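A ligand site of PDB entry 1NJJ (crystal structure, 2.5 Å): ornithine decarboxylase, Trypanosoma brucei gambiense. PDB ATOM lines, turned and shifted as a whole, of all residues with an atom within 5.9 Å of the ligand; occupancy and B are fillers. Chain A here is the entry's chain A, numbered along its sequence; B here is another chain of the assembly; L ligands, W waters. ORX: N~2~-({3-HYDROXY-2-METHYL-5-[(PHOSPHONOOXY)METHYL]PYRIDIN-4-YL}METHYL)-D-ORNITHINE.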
ATOM      1  N   ALA A  67       2.386  10.511   5.778  1.00  0.00           N
ATOM      2  CA  ALA A  67       2.374  11.701   4.925  1.00  0.00           C
ATOM      3  C   ALA A  67       3.608  11.685   4.019  1.00  0.00           C
ATOM      4  O   ALA A  67       4.640  12.235   4.359  1.00  0.00           O
ATOM      5  CB  ALA A  67       2.377  12.946   5.802  1.00  0.00           C
ATOM      6  N   LYS A  69       4.680  13.339   1.720  1.00  0.00           N
ATOM      7  CA  LYS A  69       5.300  14.648   1.487  1.00  0.00           C
ATOM      8  C   LYS A  69       6.514  14.895   2.376  1.00  0.00           C
ATOM      9  O   LYS A  69       7.431  15.635   1.999  1.00  0.00           O
ATOM     10  CB  LYS A  69       4.271  15.749   1.746  1.00  0.00           C
ATOM     11  CG  LYS A  69       4.061  16.011   3.244  1.00  0.00           C
ATOM     12  CD  LYS A  69       2.718  16.675   3.559  1.00  0.00           C
ATOM     13  CE  LYS A  69       1.559  15.711   3.328  1.00  0.00           C
ATOM     14  NZ  LYS A  69       0.252  16.286   3.736  1.00  0.00           N
ATOM     15  N   CYS A  70       6.509  14.294   3.564  1.00  0.00           N
ATOM     16  CA  CYS A  70       7.585  14.479   4.538  1.00  0.00           C
ATOM     17  C   CYS A  70       8.940  13.951   4.093  1.00  0.00           C
ATOM     18  O   CYS A  70       9.974  14.561   4.379  1.00  0.00           O
ATOM     19  CB  CYS A  70       7.204  13.806   5.849  1.00  0.00           C
ATOM     20  SG  CYS A  70       8.305  14.204   7.216  1.00  0.00           S
ATOM     21  N   ASP A  88      -0.529   8.610   3.186  1.00  0.00           N
ATOM     22  CA  ASP A  88      -1.266   9.848   2.980  1.00  0.00           C
ATOM     23  C   ASP A  88      -0.651  10.620   1.812  1.00  0.00           C
ATOM     24  O   ASP A  88       0.304  11.368   2.002  1.00  0.00           O
ATOM     25  CB  ASP A  88      -1.222  10.724   4.228  1.00  0.00           C
ATOM     26  CG  ASP A  88      -1.648  12.150   3.951  1.00  0.00           C
ATOM     27  OD1 ASP A  88      -2.215  12.401   2.875  1.00  0.00           O
ATOM     28  OD2 ASP A  88      -1.424  13.023   4.826  1.00  0.00           O
ATOM     29  N   ALA A 111      -5.305  12.980   0.941  1.00  0.00           N
ATOM     30  CA  ALA A 111      -5.616  13.967   1.964  1.00  0.00           C
ATOM     31  C   ALA A 111      -5.425  15.444   1.648  1.00  0.00           C
ATOM     32  O   ALA A 111      -5.246  16.263   2.554  1.00  0.00           O
ATOM     33  CB  ALA A 111      -4.874  13.619   3.236  1.00  0.00           C
ATOM     34  N   ARG A 154     -12.639  17.690   6.433  1.00  0.00           N
ATOM     35  CA  ARG A 154     -11.601  18.212   7.302  1.00  0.00           C
ATOM     36  C   ARG A 154     -12.063  19.498   7.957  1.00  0.00           C
ATOM     37  O   ARG A 154     -12.570  20.383   7.291  1.00  0.00           O
ATOM     38  CB  ARG A 154     -10.320  18.472   6.504  1.00  0.00           C
ATOM     39  CG  ARG A 154      -9.230  19.145   7.315  1.00  0.00           C
ATOM     40  CD  ARG A 154      -7.918  19.215   6.559  1.00  0.00           C
ATOM     41  NE  ARG A 154      -6.998  20.154   7.206  1.00  0.00           N
ATOM     42  CZ  ARG A 154      -5.764  20.399   6.794  1.00  0.00           C
ATOM     43  NH1 ARG A 154      -5.284  19.777   5.723  1.00  0.00           N
ATOM     44  NH2 ARG A 154      -5.015  21.289   7.444  1.00  0.00           N
ATOM     45  N   HIS A 197      -6.202  18.739  11.554  1.00  0.00           N
ATOM     46  CA  HIS A 197      -4.748  18.775  11.624  1.00  0.00           C
ATOM     47  C   HIS A 197      -4.316  19.954  12.464  1.00  0.00           C
ATOM     48  O   HIS A 197      -4.655  21.101  12.162  1.00  0.00           O
ATOM     49  CB  HIS A 197      -4.156  18.899  10.229  1.00  0.00           C
ATOM     50  CG  HIS A 197      -2.706  18.586  10.175  1.00  0.00           C
ATOM     51  ND1 HIS A 197      -1.749  19.364  10.797  1.00  0.00           N
ATOM     52  CD2 HIS A 197      -2.033  17.545   9.636  1.00  0.00           C
ATOM     53  CE1 HIS A 197      -0.558  18.827  10.631  1.00  0.00           C
ATOM     54  NE2 HIS A 197      -0.701  17.716   9.929  1.00  0.00           N
ATOM     55  N   GLY A 199      -0.949  20.366  13.391  1.00  0.00           N
ATOM     56  CA  GLY A 199       0.391  20.761  12.971  1.00  0.00           C
ATOM     57  C   GLY A 199       1.409  20.457  14.050  1.00  0.00           C
ATOM     58  O   GLY A 199       1.066  19.948  15.119  1.00  0.00           O
ATOM     59  N   SER A 200       2.670  20.791  13.779  1.00  0.00           N
ATOM     60  CA  SER A 200       3.752  20.522  14.726  1.00  0.00           C
ATOM     61  C   SER A 200       4.095  21.676  15.664  1.00  0.00           C
ATOM     62  O   SER A 200       4.901  21.519  16.583  1.00  0.00           O
ATOM     63  CB  SER A 200       5.002  20.096  13.953  1.00  0.00           C
ATOM     64  OG  SER A 200       5.247  20.944  12.850  1.00  0.00           O
ATOM     65  N   GLY A 235      -5.056  13.492  11.717  1.00  0.00           N
ATOM     66  CA  GLY A 235      -3.950  14.213  11.110  1.00  0.00           C
ATOM     67  C   GLY A 235      -2.538  13.848  11.506  1.00  0.00           C
ATOM     68  O   GLY A 235      -2.198  12.672  11.710  1.00  0.00           O
ATOM     69  N   GLY A 236      -1.692  14.880  11.609  1.00  0.00           N
ATOM     70  CA  GLY A 236      -0.304  14.675  11.964  1.00  0.00           C
ATOM     71  C   GLY A 236       0.224  15.728  12.912  1.00  0.00           C
ATOM     72  O   GLY A 236      -0.550  16.368  13.627  1.00  0.00           O
ATOM     73  N   GLY A 237       1.540  15.896  12.936  1.00  0.00           N
ATOM     74  CA  GLY A 237       2.134  16.883  13.815  1.00  0.00           C
ATOM     75  C   GLY A 237       2.780  16.260  15.043  1.00  0.00           C
ATOM     76  O   GLY A 237       3.034  16.949  16.052  1.00  0.00           O
ATOM     77  N   PHE A 238       3.058  14.961  14.968  1.00  0.00           N
ATOM     78  CA  PHE A 238       3.668  14.252  16.077  1.00  0.00           C
ATOM     79  C   PHE A 238       5.185  14.314  16.051  1.00  0.00           C
ATOM     80  O   PHE A 238       5.815  14.017  15.030  1.00  0.00           O
ATOM     81  CB  PHE A 238       3.225  12.777  16.096  1.00  0.00           C
ATOM     82  CG  PHE A 238       1.751  12.590  15.901  1.00  0.00           C
ATOM     83  CD1 PHE A 238       1.235  12.329  14.631  1.00  0.00           C
ATOM     84  CD2 PHE A 238       0.871  12.672  16.972  1.00  0.00           C
ATOM     85  CE1 PHE A 238      -0.125  12.171  14.441  1.00  0.00           C
ATOM     86  CE2 PHE A 238      -0.496  12.509  16.798  1.00  0.00           C
ATOM     87  CZ  PHE A 238      -0.990  12.253  15.532  1.00  0.00           C
ATOM     88  N   GLU A 274      -2.404  10.932  10.007  1.00  0.00           N
ATOM     89  CA  GLU A 274      -1.506  11.229   8.899  1.00  0.00           C
ATOM     90  C   GLU A 274      -0.159  11.677   9.468  1.00  0.00           C
ATOM     91  O   GLU A 274       0.225  12.843   9.365  1.00  0.00           O
ATOM     92  CB  GLU A 274      -2.092  12.362   8.037  1.00  0.00           C
ATOM     93  CG  GLU A 274      -3.322  11.977   7.250  1.00  0.00           C
ATOM     94  CD  GLU A 274      -4.268  13.151   7.045  1.00  0.00           C
ATOM     95  OE1 GLU A 274      -5.236  12.995   6.270  1.00  0.00           O
ATOM     96  OE2 GLU A 274      -4.064  14.219   7.670  1.00  0.00           O
ATOM     97  N   PRO A 275       0.579  10.753  10.093  1.00  0.00           N
ATOM     98  CA  PRO A 275       1.880  11.121  10.657  1.00  0.00           C
ATOM     99  C   PRO A 275       2.941  11.278   9.572  1.00  0.00           C
ATOM    100  O   PRO A 275       3.053  10.465   8.650  1.00  0.00           O
ATOM    101  CB  PRO A 275       2.158   9.969  11.610  1.00  0.00           C
ATOM    102  CG  PRO A 275       1.617   8.795  10.848  1.00  0.00           C
ATOM    103  CD  PRO A 275       0.285   9.330  10.347  1.00  0.00           C
ATOM    104  N   GLY A 276       3.735  12.343   9.694  1.00  0.00           N
ATOM    105  CA  GLY A 276       4.790  12.576   8.719  1.00  0.00           C
ATOM    106  C   GLY A 276       6.180  12.525   9.315  1.00  0.00           C
ATOM    107  O   GLY A 276       6.941  11.589   9.067  1.00  0.00           O
ATOM    108  N   ARG A 277       6.507  13.539  10.120  1.00  0.00           N
ATOM    109  CA  ARG A 277       7.822  13.633  10.740  1.00  0.00           C
ATOM    110  C   ARG A 277       8.073  12.576  11.820  1.00  0.00           C
ATOM    111  O   ARG A 277       9.209  12.169  12.046  1.00  0.00           O
ATOM    112  CB  ARG A 277       8.017  15.046  11.320  1.00  0.00           C
ATOM    113  CG  ARG A 277       6.996  15.457  12.349  1.00  0.00           C
ATOM    114  CD  ARG A 277       7.286  16.838  12.940  1.00  0.00           C
ATOM    115  NE  ARG A 277       6.763  17.935  12.107  1.00  0.00           N
ATOM    116  CZ  ARG A 277       7.438  18.547  11.133  1.00  0.00           C
ATOM    117  NH1 ARG A 277       8.688  18.192  10.856  1.00  0.00           N
ATOM    118  NH2 ARG A 277       6.854  19.511  10.436  1.00  0.00           N
ATOM    119  N   TYR A 278       7.003  12.135  12.486  1.00  0.00           N
ATOM    120  CA  TYR A 278       7.127  11.118  13.522  1.00  0.00           C
ATOM    121  C   TYR A 278       7.947   9.916  13.045  1.00  0.00           C
ATOM    122  O   TYR A 278       8.842   9.446  13.748  1.00  0.00           O
ATOM    123  CB  TYR A 278       5.746  10.621  13.959  1.00  0.00           C
ATOM    124  CG  TYR A 278       5.804   9.440  14.906  1.00  0.00           C
ATOM    125  CD1 TYR A 278       5.871   9.628  16.286  1.00  0.00           C
ATOM    126  CD2 TYR A 278       5.884   8.138  14.407  1.00  0.00           C
ATOM    127  CE1 TYR A 278       6.036   8.541  17.150  1.00  0.00           C
ATOM    128  CE2 TYR A 278       6.043   7.039  15.265  1.00  0.00           C
ATOM    129  CZ  TYR A 278       6.120   7.249  16.643  1.00  0.00           C
ATOM    130  OH  TYR A 278       6.321   6.177  17.494  1.00  0.00           O
ATOM    131  N   TYR A 331      11.621  26.636   5.089  1.00  0.00           N
ATOM    132  CA  TYR A 331      10.304  26.023   4.875  1.00  0.00           C
ATOM    133  C   TYR A 331       9.684  25.346   6.095  1.00  0.00           C
ATOM    134  O   TYR A 331       8.466  25.399   6.276  1.00  0.00           O
ATOM    135  CB  TYR A 331      10.384  24.996   3.740  1.00  0.00           C
ATOM    136  CG  TYR A 331      10.399  25.609   2.365  1.00  0.00           C
ATOM    137  CD1 TYR A 331      11.375  25.258   1.431  1.00  0.00           C
ATOM    138  CD2 TYR A 331       9.430  26.524   1.976  1.00  0.00           C
ATOM    139  CE1 TYR A 331      11.396  25.813   0.164  1.00  0.00           C
ATOM    140  CE2 TYR A 331       9.430  27.075   0.706  1.00  0.00           C
ATOM    141  CZ  TYR A 331      10.413  26.720  -0.193  1.00  0.00           C
ATOM    142  OH  TYR A 331      10.429  27.288  -1.445  1.00  0.00           O
ATOM    143  N   ASP A 332      10.501  24.715   6.938  1.00  0.00           N
ATOM    144  CA  ASP A 332       9.962  24.007   8.093  1.00  0.00           C
ATOM    145  C   ASP A 332      10.358  24.490   9.480  1.00  0.00           C
ATOM    146  O   ASP A 332      10.159  23.765  10.464  1.00  0.00           O
ATOM    147  CB  ASP A 332      10.314  22.521   7.975  1.00  0.00           C
ATOM    148  CG  ASP A 332       9.397  21.629   8.795  1.00  0.00           C
ATOM    149  OD1 ASP A 332       9.759  20.457   9.003  1.00  0.00           O
ATOM    150  OD2 ASP A 332       8.320  22.105   9.215  1.00  0.00           O
ATOM    151  N   TYR A 389      11.190  16.477   5.866  1.00  0.00           N
ATOM    152  CA  TYR A 389      11.115  17.645   4.980  1.00  0.00           C
ATOM    153  C   TYR A 389      12.495  18.188   4.640  1.00  0.00           C
ATOM    154  O   TYR A 389      12.785  19.371   4.834  1.00  0.00           O
ATOM    155  CB  TYR A 389      10.287  18.753   5.634  1.00  0.00           C
ATOM    156  CG  TYR A 389       8.895  18.301   6.028  1.00  0.00           C
ATOM    157  CD1 TYR A 389       8.480  18.315   7.357  1.00  0.00           C
ATOM    158  CD2 TYR A 389       8.008  17.834   5.059  1.00  0.00           C
ATOM    159  CE1 TYR A 389       7.221  17.872   7.727  1.00  0.00           C
ATOM    160  CE2 TYR A 389       6.746  17.373   5.415  1.00  0.00           C
ATOM    161  CZ  TYR A 389       6.353  17.392   6.749  1.00  0.00           C
ATOM    162  OH  TYR A 389       5.113  16.928   7.088  1.00  0.00           O
ATOM    163  N   TYR B 323       6.834  25.962  -3.352  1.00  0.00           N
ATOM    164  CA  TYR B 323       7.715  24.808  -3.554  1.00  0.00           C
ATOM    165  C   TYR B 323       8.078  24.690  -5.022  1.00  0.00           C
ATOM    166  O   TYR B 323       8.473  23.633  -5.503  1.00  0.00           O
ATOM    167  CB  TYR B 323       7.056  23.510  -3.082  1.00  0.00           C
ATOM    168  CG  TYR B 323       7.011  23.375  -1.584  1.00  0.00           C
ATOM    169  CD1 TYR B 323       6.070  24.061  -0.836  1.00  0.00           C
ATOM    170  CD2 TYR B 323       7.959  22.605  -0.901  1.00  0.00           C
ATOM    171  CE1 TYR B 323       6.066  24.004   0.552  1.00  0.00           C
ATOM    172  CE2 TYR B 323       7.971  22.542   0.485  1.00  0.00           C
ATOM    173  CZ  TYR B 323       7.028  23.243   1.204  1.00  0.00           C
ATOM    174  OH  TYR B 323       7.040  23.231   2.574  1.00  0.00           O
ATOM    175  N   CYS B 360      -0.127  21.148   0.676  1.00  0.00           N
ATOM    176  CA  CYS B 360      -0.784  21.087   1.991  1.00  0.00           C
ATOM    177  C   CYS B 360      -0.132  22.005   3.038  1.00  0.00           C
ATOM    178  O   CYS B 360      -0.661  22.162   4.139  1.00  0.00           O
ATOM    179  CB  CYS B 360      -0.787  19.654   2.537  1.00  0.00           C
ATOM    180  SG  CYS B 360      -1.921  18.513   1.706  1.00  0.00           S
ATOM    181  N   ASP B 361       1.002  22.595   2.684  1.00  0.00           N
ATOM    182  CA  ASP B 361       1.717  23.473   3.596  1.00  0.00           C
ATOM    183  C   ASP B 361       0.989  24.816   3.705  1.00  0.00           C
ATOM    184  O   ASP B 361       0.756  25.482   2.700  1.00  0.00           O
ATOM    185  CB  ASP B 361       3.138  23.697   3.082  1.00  0.00           C
ATOM    186  CG  ASP B 361       4.043  24.374   4.095  1.00  0.00           C
ATOM    187  OD1 ASP B 361       3.608  25.377   4.705  1.00  0.00           O
ATOM    188  OD2 ASP B 361       5.188  23.906   4.281  1.00  0.00           O
ATOM    189  N   GLY B 362       0.619  25.203   4.917  1.00  0.00           N
ATOM    190  CA  GLY B 362      -0.075  26.457   5.118  1.00  0.00           C
ATOM    191  C   GLY B 362       0.793  27.670   4.873  1.00  0.00           C
ATOM    192  O   GLY B 362       0.331  28.813   4.972  1.00  0.00           O
ATOM    193  N   LEU B 363       2.064  27.428   4.574  1.00  0.00           N
ATOM    194  CA  LEU B 363       3.025  28.490   4.318  1.00  0.00           C
ATOM    195  C   LEU B 363       3.069  28.700   2.809  1.00  0.00           C
ATOM    196  O   LEU B 363       3.525  29.730   2.326  1.00  0.00           O
ATOM    197  CB  LEU B 363       4.415  28.075   4.833  1.00  0.00           C
ATOM    198  CG  LEU B 363       5.634  28.894   4.421  1.00  0.00           C
ATOM    199  CD1 LEU B 363       5.792  30.109   5.329  1.00  0.00           C
ATOM    200  CD2 LEU B 363       6.880  28.009   4.501  1.00  0.00           C
HETATM  201  OA  ORX L   1       2.155  23.236   7.636  1.00  0.00           O
HETATM  202  CA  ORX L   1       2.296  21.895   7.809  1.00  0.00           C
HETATM  203  OXT ORX L   1       1.805  21.317   8.951  1.00  0.00           O
HETATM  204  CAA ORX L   1       3.013  21.046   6.727  1.00  0.00           C
HETATM  205  NA  ORX L   1       2.181  19.764   6.336  1.00  0.00           N
HETATM  206  C4A ORX L   1       2.027  18.763   7.485  1.00  0.00           C
HETATM  207  C4  ORX L   1       0.872  17.717   7.259  1.00  0.00           C
HETATM  208  C5  ORX L   1       0.937  16.338   7.700  1.00  0.00           C
HETATM  209  C6  ORX L   1      -0.016  15.349   7.545  1.00  0.00           C
HETATM  210  N1  ORX L   1      -1.202  15.637   6.917  1.00  0.00           N
HETATM  211  C2  ORX L   1      -1.443  16.924   6.431  1.00  0.00           C
HETATM  212  C3  ORX L   1      -0.389  17.967   6.607  1.00  0.00           C
HETATM  213  O3  ORX L   1      -0.767  19.161   6.093  1.00  0.00           O
HETATM  214  C2A ORX L   1      -2.833  16.927   5.795  1.00  0.00           C
HETATM  215  C5A ORX L   1       2.132  15.812   8.418  1.00  0.00           C
HETATM  216  OP4 ORX L   1       2.572  16.574   9.464  1.00  0.00           O
HETATM  217  P   ORX L   1       3.738  16.067  10.377  1.00  0.00           P
HETATM  218  OP1 ORX L   1       4.079  17.034  11.382  1.00  0.00           O
HETATM  219  OP2 ORX L   1       4.793  15.575   9.390  1.00  0.00           O
HETATM  220  OP3 ORX L   1       3.115  14.917  11.137  1.00  0.00           O
HETATM  221  CBA ORX L   1       4.465  20.787   7.198  1.00  0.00           C
HETATM  222  CGA ORX L   1       5.477  21.883   6.876  1.00  0.00           C
HETATM  223  CDA ORX L   1       6.643  21.348   6.042  1.00  0.00           C
HETATM  224  NE  ORX L   1       7.612  22.440   5.804  1.00  0.00           N
HETATM  225  O   HOH W   1       8.894  21.289   3.652  1.00  0.00           O
HETATM  226  O   HOH W   2       4.562  13.319  12.656  1.00  0.00           O
HETATM  227  O   HOH W   3      -2.828  21.634   5.870  1.00  0.00           O
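The backbone NH (N) of Gly 276 sits at hydrogen-bond distance from an oxygen (OP3) of the ligand (3.0 Å). OD2 of Asp 332 is in salt-bridge range of NE of the ligand (3.5 Å). A ring nitrogen (NE2) of His 197 lies close to an oxygen (OP4) of the ligand, at 3.5 Å. A nitrogen (NE) of the ligand is in hydrogen-bond range of the side-chain hydroxyl (OH) of Tyr 323 of chain B (3.4 Å). NE of the ligand is in salt-bridge range of OD2 of Asp 361 of chain B. The side-chain hydroxyl (OH) of Tyr 389 is in hydrogen-bond range of an oxygen (OP2) of the ligand, at 2.7 Å. An oxygen (OP2) of the ligand lies within hydrogen-bond range of the backbone NH of Arg 277, at 2.8 Å. The guanidinium group (NE) of Arg 277 lies within salt-bridge range of an oxygen (OP1) of the ligand (2.9 Å). A nitrogen (NE) of the ligand lies within hydrogen-bond range of the backbone carbonyl oxygen of Tyr 331 (3.1 Å). The backbone NH of Gly 237 lies within hydrogen-bond range of an oxygen (OP3) of the ligand (2.6 Å).
The backbone NH (N) of Ala 67 lies within hydrogen-bond range of the backbone carbonyl oxygen (O) of Pro 275 (2.9 Å). The side-chain carboxylate of Asp 361 of chain B lies within hydrogen-bond range of the backbone NH of Leu 363 of chain B (2.6 Å). The backbone carbonyl oxygen of Cys 70 is in hydrogen-bond range of the backbone NH of Tyr 389 (2.7 Å). The backbone NH of Gly 199 is in hydrogen-bond range of a ring nitrogen (ND1) of His 197 (2.9 Å). OD2 of Asp 361 of chain B lies within hydrogen-bond range of OH of Tyr 323 of chain B (2.6 Å). The side-chain hydroxyl (OG) of Ser 200 is in hydrogen-bond range of the guanidinium group (NH2) of Arg 277 (3.2 Å). OD1 of Asp 332 is in salt-bridge range of NH1 of Arg 277, at 3.1 Å. O of Gly 276 lies close to SG of Cys 70 (3.5 Å).
The side-chain carboxylate (OD2) of Asp 88 sits close to a nitrogen (N1) of the ligand, 3.4 Å away. OE2 of Glu 274 sits close to N1 of the ligand (3.3 Å). Residues that only touch the ligand: Lys 69, Gly 236, Cys 360 of chain B, Gly 362 of chain B, Arg 154, Ala 67, Phe 238 and Pro 275.
Water W1 lies within hydrogen-bond range of NE of the ligand (2.8 Å) and OH of Tyr 323 of chain B (2.9 Å). Water W3 lies within hydrogen-bond range of the guanidinium group of Arg 154 (2.7 Å), the backbone carbonyl oxygen of Cys 360 of chain B (2.8 Å) and an oxygen (O3) of the ligand (3.2 Å).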
